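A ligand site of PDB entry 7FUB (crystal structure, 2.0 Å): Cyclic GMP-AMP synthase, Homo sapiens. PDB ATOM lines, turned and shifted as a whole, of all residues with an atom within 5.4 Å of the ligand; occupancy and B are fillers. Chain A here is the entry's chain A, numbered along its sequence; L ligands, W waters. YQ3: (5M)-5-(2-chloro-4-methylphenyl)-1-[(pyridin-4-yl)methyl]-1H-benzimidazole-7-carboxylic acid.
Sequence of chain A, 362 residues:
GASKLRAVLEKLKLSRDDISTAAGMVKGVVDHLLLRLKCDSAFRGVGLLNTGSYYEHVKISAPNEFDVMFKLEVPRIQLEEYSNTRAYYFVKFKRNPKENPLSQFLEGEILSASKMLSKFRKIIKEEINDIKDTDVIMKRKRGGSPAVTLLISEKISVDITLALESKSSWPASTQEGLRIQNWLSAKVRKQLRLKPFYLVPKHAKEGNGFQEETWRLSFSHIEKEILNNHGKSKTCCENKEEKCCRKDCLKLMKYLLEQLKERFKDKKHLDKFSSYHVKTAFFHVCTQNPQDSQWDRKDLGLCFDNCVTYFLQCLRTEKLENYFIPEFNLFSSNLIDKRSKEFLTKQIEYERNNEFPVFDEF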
ATOM      1  N   LYS A  59      22.740 -18.873   2.622  1.00  0.00           N
ATOM      2  CA  LYS A  59      22.268 -19.990   3.445  1.00  0.00           C
ATOM      3  C   LYS A  59      22.573 -21.300   2.717  1.00  0.00           C
ATOM      4  O   LYS A  59      22.417 -21.393   1.495  1.00  0.00           O
ATOM      5  CB  LYS A  59      20.764 -19.829   3.704  1.00  0.00           C
ATOM      6  CG  LYS A  59      20.198 -20.600   4.885  1.00  0.00           C
ATOM      7  CD  LYS A  59      18.665 -20.435   5.026  1.00  0.00           C
ATOM      8  CE  LYS A  59      18.262 -19.470   6.170  1.00  0.00           C
ATOM      9  NZ  LYS A  59      16.892 -19.706   6.777  1.00  0.00           N
ATOM     10  N   ASP A  67      21.106 -21.172  -0.862  1.00  0.00           N
ATOM     11  CA  ASP A  67      19.886 -20.386  -0.951  1.00  0.00           C
ATOM     12  C   ASP A  67      20.225 -18.937  -0.626  1.00  0.00           C
ATOM     13  O   ASP A  67      20.800 -18.641   0.430  1.00  0.00           O
ATOM     14  CB  ASP A  67      18.803 -20.884   0.021  1.00  0.00           C
ATOM     15  CG  ASP A  67      18.116 -22.163  -0.464  1.00  0.00           C
ATOM     16  OD1 ASP A  67      18.526 -22.731  -1.502  1.00  0.00           O
ATOM     17  OD2 ASP A  67      17.157 -22.587   0.216  1.00  0.00           O
ATOM     18  N   PRO A 146       9.777 -20.437  -6.335  1.00  0.00           N
ATOM     19  CA  PRO A 146      10.208 -19.038  -6.403  1.00  0.00           C
ATOM     20  C   PRO A 146      11.656 -18.876  -6.829  1.00  0.00           C
ATOM     21  O   PRO A 146      12.112 -17.738  -7.004  1.00  0.00           O
ATOM     22  CB  PRO A 146      10.021 -18.557  -4.957  1.00  0.00           C
ATOM     23  CG  PRO A 146       9.941 -19.846  -4.098  1.00  0.00           C
ATOM     24  CD  PRO A 146      10.080 -21.027  -5.019  1.00  0.00           C
ATOM     25  N   LEU A 178       4.829 -19.465  15.734  1.00  0.00           N
ATOM     26  CA  LEU A 178       6.016 -19.059  16.493  1.00  0.00           C
ATOM     27  C   LEU A 178       5.772 -19.257  17.991  1.00  0.00           C
ATOM     28  O   LEU A 178       5.815 -18.306  18.777  1.00  0.00           O
ATOM     29  CB  LEU A 178       6.398 -17.607  16.189  1.00  0.00           C
ATOM     30  CG  LEU A 178       7.816 -17.102  16.489  1.00  0.00           C
ATOM     31  CD1 LEU A 178       8.813 -17.954  15.764  1.00  0.00           C
ATOM     32  CD2 LEU A 178       7.963 -15.669  16.042  1.00  0.00           C
ATOM     33  N   VAL A 200       7.144 -14.656  -1.224  1.00  0.00           N
ATOM     34  CA  VAL A 200       7.952 -15.219  -2.293  1.00  0.00           C
ATOM     35  C   VAL A 200       7.000 -15.814  -3.314  1.00  0.00           C
ATOM     36  O   VAL A 200       5.954 -16.356  -2.945  1.00  0.00           O
ATOM     37  CB  VAL A 200       8.967 -16.240  -1.757  1.00  0.00           C
ATOM     38  CG1 VAL A 200       9.915 -15.549  -0.812  1.00  0.00           C
ATOM     39  CG2 VAL A 200       8.250 -17.401  -1.071  1.00  0.00           C
ATOM     40  N   LYS A 202       6.176 -18.440  -4.829  1.00  0.00           N
ATOM     41  CA  LYS A 202       5.855 -19.847  -4.974  1.00  0.00           C
ATOM     42  C   LYS A 202       4.358 -19.974  -5.198  1.00  0.00           C
ATOM     43  O   LYS A 202       3.557 -19.280  -4.568  1.00  0.00           O
ATOM     44  CB  LYS A 202       6.271 -20.650  -3.735  1.00  0.00           C
ATOM     45  CG  LYS A 202       5.843 -22.106  -3.751  1.00  0.00           C
ATOM     46  CD  LYS A 202       6.882 -22.994  -3.075  1.00  0.00           C
ATOM     47  CE  LYS A 202       6.275 -24.239  -2.436  1.00  0.00           C
ATOM     48  NZ  LYS A 202       7.292 -25.042  -1.686  1.00  0.00           N
ATOM     49  N   ARG A 216       3.701 -16.706  -1.410  1.00  0.00           N
ATOM     50  CA  ARG A 216       3.729 -17.515  -0.200  1.00  0.00           C
ATOM     51  C   ARG A 216       4.461 -16.749   0.891  1.00  0.00           C
ATOM     52  O   ARG A 216       5.547 -16.240   0.638  1.00  0.00           O
ATOM     53  CB  ARG A 216       4.448 -18.836  -0.481  1.00  0.00           C
ATOM     54  CG  ARG A 216       4.639 -19.744   0.713  1.00  0.00           C
ATOM     55  CD  ARG A 216       5.611 -20.830   0.330  1.00  0.00           C
ATOM     56  NE  ARG A 216       5.466 -22.031   1.146  1.00  0.00           N
ATOM     57  CZ  ARG A 216       5.994 -22.189   2.360  1.00  0.00           C
ATOM     58  NH1 ARG A 216       6.687 -21.213   2.928  1.00  0.00           N
ATOM     59  NH2 ARG A 216       5.810 -23.337   3.009  1.00  0.00           N
ATOM     60  N   LEU A 217       3.869 -16.688   2.090  1.00  0.00           N
ATOM     61  CA  LEU A 217       4.547 -16.075   3.239  1.00  0.00           C
ATOM     62  C   LEU A 217       5.875 -16.747   3.504  1.00  0.00           C
ATOM     63  O   LEU A 217       5.975 -17.982   3.515  1.00  0.00           O
ATOM     64  CB  LEU A 217       3.683 -16.190   4.489  1.00  0.00           C
ATOM     65  CG  LEU A 217       2.434 -15.324   4.597  1.00  0.00           C
ATOM     66  CD1 LEU A 217       1.741 -15.566   5.899  1.00  0.00           C
ATOM     67  CD2 LEU A 217       2.820 -13.886   4.476  1.00  0.00           C
ATOM     68  N   SER A 218       6.912 -15.943   3.763  1.00  0.00           N
ATOM     69  CA  SER A 218       8.241 -16.464   4.049  1.00  0.00           C
ATOM     70  C   SER A 218       8.786 -15.824   5.309  1.00  0.00           C
ATOM     71  O   SER A 218       8.691 -14.602   5.482  1.00  0.00           O
ATOM     72  CB  SER A 218       9.198 -16.216   2.884  1.00  0.00           C
ATOM     73  OG  SER A 218      10.481 -16.769   3.147  1.00  0.00           O
ATOM     74  N   PHE A 219       9.370 -16.654   6.189  1.00  0.00           N
ATOM     75  CA  PHE A 219       9.941 -16.194   7.450  1.00  0.00           C
ATOM     76  C   PHE A 219      11.370 -16.703   7.643  1.00  0.00           C
ATOM     77  O   PHE A 219      11.905 -16.652   8.749  1.00  0.00           O
ATOM     78  CB  PHE A 219       9.051 -16.606   8.625  1.00  0.00           C
ATOM     79  CG  PHE A 219       7.672 -15.984   8.604  1.00  0.00           C
ATOM     80  CD1 PHE A 219       7.468 -14.716   9.113  1.00  0.00           C
ATOM     81  CD2 PHE A 219       6.591 -16.679   8.092  1.00  0.00           C
ATOM     82  CE1 PHE A 219       6.211 -14.140   9.109  1.00  0.00           C
ATOM     83  CE2 PHE A 219       5.334 -16.105   8.071  1.00  0.00           C
ATOM     84  CZ  PHE A 219       5.145 -14.842   8.586  1.00  0.00           C
ATOM     85  N   SER A 220      11.985 -17.177   6.558  1.00  0.00           N
ATOM     86  CA  SER A 220      13.349 -17.676   6.504  1.00  0.00           C
ATOM     87  C   SER A 220      14.350 -16.854   7.312  1.00  0.00           C
ATOM     88  O   SER A 220      15.266 -17.401   7.938  1.00  0.00           O
ATOM     89  CB  SER A 220      13.817 -17.721   5.048  1.00  0.00           C
ATOM     90  OG  SER A 220      15.220 -17.506   4.966  1.00  0.00           O
ATOM     91  N   ILE A 222      13.978 -15.341  10.024  1.00  0.00           N
ATOM     92  CA  ILE A 222      13.902 -15.485  11.472  1.00  0.00           C
ATOM     93  C   ILE A 222      14.835 -16.597  11.962  1.00  0.00           C
ATOM     94  O   ILE A 222      15.211 -16.609  13.138  1.00  0.00           O
ATOM     95  CB  ILE A 222      12.457 -15.761  11.912  1.00  0.00           C
ATOM     96  CG1 ILE A 222      11.494 -14.712  11.351  1.00  0.00           C
ATOM     97  CG2 ILE A 222      12.322 -15.816  13.416  1.00  0.00           C
ATOM     98  CD1 ILE A 222      11.693 -13.309  11.870  1.00  0.00           C
ATOM     99  N   GLU A 223      15.259 -17.505  11.084  1.00  0.00           N
ATOM    100  CA  GLU A 223      15.997 -18.669  11.549  1.00  0.00           C
ATOM    101  C   GLU A 223      17.290 -18.278  12.243  1.00  0.00           C
ATOM    102  O   GLU A 223      17.528 -18.691  13.376  1.00  0.00           O
ATOM    103  CB  GLU A 223      16.290 -19.616  10.388  1.00  0.00           C
ATOM    104  CG  GLU A 223      16.724 -20.979  10.915  1.00  0.00           C
ATOM    105  CD  GLU A 223      17.369 -21.855   9.853  1.00  0.00           C
ATOM    106  OE1 GLU A 223      17.206 -21.538   8.653  1.00  0.00           O
ATOM    107  OE2 GLU A 223      18.023 -22.862  10.235  1.00  0.00           O
ATOM    108  N   ILE A 226      16.956 -17.044  15.806  1.00  0.00           N
ATOM    109  CA  ILE A 226      16.696 -17.988  16.885  1.00  0.00           C
ATOM    110  C   ILE A 226      17.818 -19.022  17.004  1.00  0.00           C
ATOM    111  O   ILE A 226      18.138 -19.463  18.123  1.00  0.00           O
ATOM    112  CB  ILE A 226      15.331 -18.684  16.670  1.00  0.00           C
ATOM    113  CG1 ILE A 226      14.229 -17.668  16.982  1.00  0.00           C
ATOM    114  CG2 ILE A 226      15.258 -19.920  17.537  1.00  0.00           C
ATOM    115  CD1 ILE A 226      12.842 -18.225  16.836  1.00  0.00           C
ATOM    116  N   TYR A 276      14.426 -28.005   5.035  1.00  0.00           N
ATOM    117  CA  TYR A 276      13.356 -27.197   5.617  1.00  0.00           C
ATOM    118  C   TYR A 276      12.423 -28.042   6.459  1.00  0.00           C
ATOM    119  O   TYR A 276      11.908 -27.587   7.491  1.00  0.00           O
ATOM    120  CB  TYR A 276      12.570 -26.511   4.493  1.00  0.00           C
ATOM    121  CG  TYR A 276      11.351 -25.730   4.909  1.00  0.00           C
ATOM    122  CD1 TYR A 276      11.421 -24.738   5.887  1.00  0.00           C
ATOM    123  CD2 TYR A 276      10.137 -25.945   4.287  1.00  0.00           C
ATOM    124  CE1 TYR A 276      10.267 -23.996   6.237  1.00  0.00           C
ATOM    125  CE2 TYR A 276       9.004 -25.198   4.624  1.00  0.00           C
ATOM    126  CZ  TYR A 276       9.072 -24.245   5.591  1.00  0.00           C
ATOM    127  OH  TYR A 276       7.909 -23.556   5.892  1.00  0.00           O
ATOM    128  N   LYS A 279      14.379 -28.712   9.720  1.00  0.00           N
ATOM    129  CA  LYS A 279      14.447 -27.543  10.602  1.00  0.00           C
ATOM    130  C   LYS A 279      13.130 -27.311  11.305  1.00  0.00           C
ATOM    131  O   LYS A 279      13.106 -27.063  12.518  1.00  0.00           O
ATOM    132  CB  LYS A 279      14.820 -26.271   9.825  1.00  0.00           C
ATOM    133  CG  LYS A 279      16.249 -26.144   9.212  1.00  0.00           C
ATOM    134  CD  LYS A 279      16.274 -24.902   8.275  1.00  0.00           C
ATOM    135  CE  LYS A 279      17.480 -24.789   7.367  1.00  0.00           C
ATOM    136  NZ  LYS A 279      18.734 -24.342   8.040  1.00  0.00           N
ATOM    137  N   THR A 280      12.023 -27.376  10.554  1.00  0.00           N
ATOM    138  CA  THR A 280      10.690 -27.186  11.119  1.00  0.00           C
ATOM    139  C   THR A 280      10.416 -28.170  12.246  1.00  0.00           C
ATOM    140  O   THR A 280       9.977 -27.773  13.334  1.00  0.00           O
ATOM    141  CB  THR A 280       9.640 -27.342  10.012  1.00  0.00           C
ATOM    142  OG1 THR A 280       9.792 -26.299   9.024  1.00  0.00           O
ATOM    143  CG2 THR A 280       8.238 -27.260  10.598  1.00  0.00           C
ATOM    144  N   PHE A 283      12.777 -27.219  15.407  1.00  0.00           N
ATOM    145  CA  PHE A 283      12.253 -26.103  16.199  1.00  0.00           C
ATOM    146  C   PHE A 283      10.933 -26.452  16.883  1.00  0.00           C
ATOM    147  O   PHE A 283      10.638 -25.922  17.959  1.00  0.00           O
ATOM    148  CB  PHE A 283      12.095 -24.864  15.309  1.00  0.00           C
ATOM    149  CG  PHE A 283      13.410 -24.267  14.899  1.00  0.00           C
ATOM    150  CD1 PHE A 283      14.189 -23.597  15.829  1.00  0.00           C
ATOM    151  CD2 PHE A 283      13.879 -24.406  13.606  1.00  0.00           C
ATOM    152  CE1 PHE A 283      15.408 -23.072  15.451  1.00  0.00           C
ATOM    153  CE2 PHE A 283      15.117 -23.866  13.225  1.00  0.00           C
ATOM    154  CZ  PHE A 283      15.867 -23.193  14.150  1.00  0.00           C
ATOM    155  N   ASN A 322       3.768 -25.978   9.490  1.00  0.00           N
ATOM    156  CA  ASN A 322       4.574 -24.786   9.312  1.00  0.00           C
ATOM    157  C   ASN A 322       4.772 -24.090  10.666  1.00  0.00           C
ATOM    158  O   ASN A 322       3.812 -23.883  11.416  1.00  0.00           O
ATOM    159  CB  ASN A 322       3.843 -23.892   8.296  1.00  0.00           C
ATOM    160  CG  ASN A 322       4.631 -22.669   7.884  1.00  0.00           C
ATOM    161  OD1 ASN A 322       5.066 -21.877   8.734  1.00  0.00           O
ATOM    162  ND2 ASN A 322       4.778 -22.468   6.565  1.00  0.00           N
ATOM    163  N   TYR A 323       6.031 -23.812  10.988  1.00  0.00           N
ATOM    164  CA  TYR A 323       6.375 -23.253  12.292  1.00  0.00           C
ATOM    165  C   TYR A 323       5.696 -21.925  12.530  1.00  0.00           C
ATOM    166  O   TYR A 323       5.407 -21.554  13.675  1.00  0.00           O
ATOM    167  CB  TYR A 323       7.912 -23.091  12.415  1.00  0.00           C
ATOM    168  CG  TYR A 323       8.364 -23.028  13.862  1.00  0.00           C
ATOM    169  CD1 TYR A 323       8.269 -24.134  14.677  1.00  0.00           C
ATOM    170  CD2 TYR A 323       8.883 -21.847  14.411  1.00  0.00           C
ATOM    171  CE1 TYR A 323       8.652 -24.091  15.989  1.00  0.00           C
ATOM    172  CE2 TYR A 323       9.289 -21.801  15.751  1.00  0.00           C
ATOM    173  CZ  TYR A 323       9.167 -22.934  16.531  1.00  0.00           C
ATOM    174  OH  TYR A 323       9.555 -22.966  17.868  1.00  0.00           O
ATOM    175  N   PHE A 324       5.428 -21.179  11.461  1.00  0.00           N
ATOM    176  CA  PHE A 324       4.802 -19.874  11.566  1.00  0.00           C
ATOM    177  C   PHE A 324       3.307 -19.903  11.254  1.00  0.00           C
ATOM    178  O   PHE A 324       2.570 -19.029  11.709  1.00  0.00           O
ATOM    179  CB  PHE A 324       5.530 -18.888  10.635  1.00  0.00           C
ATOM    180  CG  PHE A 324       6.932 -18.612  11.082  1.00  0.00           C
ATOM    181  CD1 PHE A 324       7.943 -19.516  10.841  1.00  0.00           C
ATOM    182  CD2 PHE A 324       7.224 -17.469  11.809  1.00  0.00           C
ATOM    183  CE1 PHE A 324       9.230 -19.278  11.287  1.00  0.00           C
ATOM    184  CE2 PHE A 324       8.478 -17.212  12.252  1.00  0.00           C
ATOM    185  CZ  PHE A 324       9.496 -18.113  11.999  1.00  0.00           C
HETATM  186  C10 YQ3 L   1      13.267 -21.660   7.530  1.00  0.00           C
HETATM  187  C11 YQ3 L   1      13.278 -21.689   6.138  1.00  0.00           C
HETATM  188  C13 YQ3 L   1      13.730 -21.967   4.074  1.00  0.00           C
HETATM  189  C15 YQ3 L   1      11.811 -20.832   2.894  1.00  0.00           C
HETATM  190  C16 YQ3 L   1      10.908 -21.799   2.178  1.00  0.00           C
HETATM  191  C17 YQ3 L   1      10.965 -23.157   2.388  1.00  0.00           C
HETATM  192  C18 YQ3 L   1      10.100 -23.980   1.693  1.00  0.00           C
HETATM  193  C20 YQ3 L   1       9.155 -22.217   0.612  1.00  0.00           C
HETATM  194  C21 YQ3 L   1       9.985 -21.320   1.260  1.00  0.00           C
HETATM  195  C22 YQ3 L   1      12.228 -21.100   5.410  1.00  0.00           C
HETATM  196  C23 YQ3 L   1      11.171 -20.484   6.114  1.00  0.00           C
HETATM  197  C24 YQ3 L   1       9.995 -19.815   5.504  1.00  0.00           C
HETATM  198  C27 YQ3 L   1      11.184 -20.471   7.513  1.00  0.00           C
HETATM  199  C1  YQ3 L   1      12.385 -20.678  14.030  1.00  0.00           C
HETATM  200  C2  YQ3 L   1      12.337 -20.790  12.526  1.00  0.00           C
HETATM  201  C3  YQ3 L   1      11.995 -21.983  11.915  1.00  0.00           C
HETATM  202  C4  YQ3 L   1      11.954 -22.088  10.545  1.00  0.00           C
HETATM  203  C6  YQ3 L   1      12.239 -21.013   9.718  1.00  0.00           C
HETATM  204  C7  YQ3 L   1      12.594 -19.808  10.337  1.00  0.00           C
HETATM  205  C8  YQ3 L   1      12.636 -19.711  11.715  1.00  0.00           C
HETATM  206  C9  YQ3 L   1      12.225 -21.058   8.230  1.00  0.00           C
HETATM  207  N12 YQ3 L   1      14.215 -22.227   5.266  1.00  0.00           N
HETATM  208  N14 YQ3 L   1      12.527 -21.319   4.072  1.00  0.00           N
HETATM  209  N19 YQ3 L   1       9.192 -23.537   0.821  1.00  0.00           N
HETATM  210  O25 YQ3 L   1       8.842 -20.058   5.876  1.00  0.00           O
HETATM  211  O26 YQ3 L   1      10.283 -18.957   4.562  1.00  0.00           O
HETATM  212 CL5  YQ3 L   1      11.512 -23.611   9.855  1.00  0.00          CL
HETATM  213  O   HOH W   1       8.127 -21.613   8.116  1.00  0.00           O
HETATM  214  O   HOH W   2       6.153 -19.530   5.995  1.00  0.00           O
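NZ of Lys 59 touches N12 of the ligand, 3.98 Å away. C of Ile 222 touches C8 of the ligand, 3.8 Å away. Glu 223 touches the ligand. CD1 of Ile 226 touches C1 of the ligand, at 3.8 Å. Tyr 276 touches the ligand (CD2 to C18, 3.3 Å). OG1 of Thr 280 touches CL5 of the ligand, at 3.3 Å. CD2 of Phe 283 touches C3 of the ligand, 3.5 Å away. CD2 of Tyr 323 touches C1 of the ligand (3.7 Å). Phe 324 touches the ligand. Hydrophobic or aromatic side chains within 4 Å of the ligand: Ile 222, Ile 226, Tyr 276, Phe 283, Tyr 323 and Phe 324. Within 4 Å of the ligand: Lys 59, Lys 202, Arg 216, Ser 218, Phe 219, Ser 220, Ile 222, Glu 223, Ile 226, Tyr 276, Thr 280, Phe 283, Tyr 323 and Phe 324. Along chain A the residues within 4 Å of the ligand span positions 59 to 324. The nearest printed residue that does not touch the ligand is Lys 279 (4.2 Å).
Water W2 lies within hydrogen-bond range of O25 of the ligand (2.7 Å), O of Leu 217 (2.9 Å) and ND2 of Asn 322 (3.3 Å). Water W1 lies within hydrogen-bond range of an oxygen (O25) of the ligand (2.8 Å), the side-chain hydroxyl (OH) of Tyr 276 (3.0 Å) and the side-chain amide oxygen (OD1) of Asn 322 (3.1 Å).
The side-chain carboxylate (OE1) of Glu 223 lies within salt-bridge range of the side-chain amino group (NZ) of Lys 59 (2.6 Å). The side-chain hydroxyl (OG1) of Thr 280 is in hydrogen-bond range of the backbone carbonyl oxygen (O) of Tyr 276. The backbone NH of Arg 216 lies within hydrogen-bond range of the backbone carbonyl oxygen of Val 200 (2.7 Å). The side-chain carboxylate (OE2) of Glu 223 is in salt-bridge range of the side-chain amino group (NZ) of Lys 279 (2.7 Å). The backbone NH (N) of Phe 324 is in hydrogen-bond range of the side-chain amide oxygen (OD1) of Asn 322. O of Tyr 323 sits at hydrogen-bond distance from N of Leu 178 (3.0 Å). The side-chain amino group (NZ) of Lys 59 sits at hydrogen-bond distance from the backbone carbonyl oxygen (O) of Ser 220. O of Lys 59 lies within hydrogen-bond range of N of Asp 67.
The backbone NH (N) of Ser 220 lies within hydrogen-bond range of an oxygen (O26) of the ligand, 3.2 Å away. The guanidinium group (NH1) of Arg 216 lies within salt-bridge range of an oxygen (O25) of the ligand, 3.8 Å away. The side-chain amino group of Lys 202 is in hydrogen-bond range of a nitrogen (N19) of the ligand. An oxygen (O26) of the ligand is in hydrogen-bond range of the side-chain hydroxyl (OG) of Ser 218, at 2.6 Å. An oxygen (O26) of the ligand sits at hydrogen-bond distance from the backbone NH (N) of Phe 219, 3.0 Å away.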
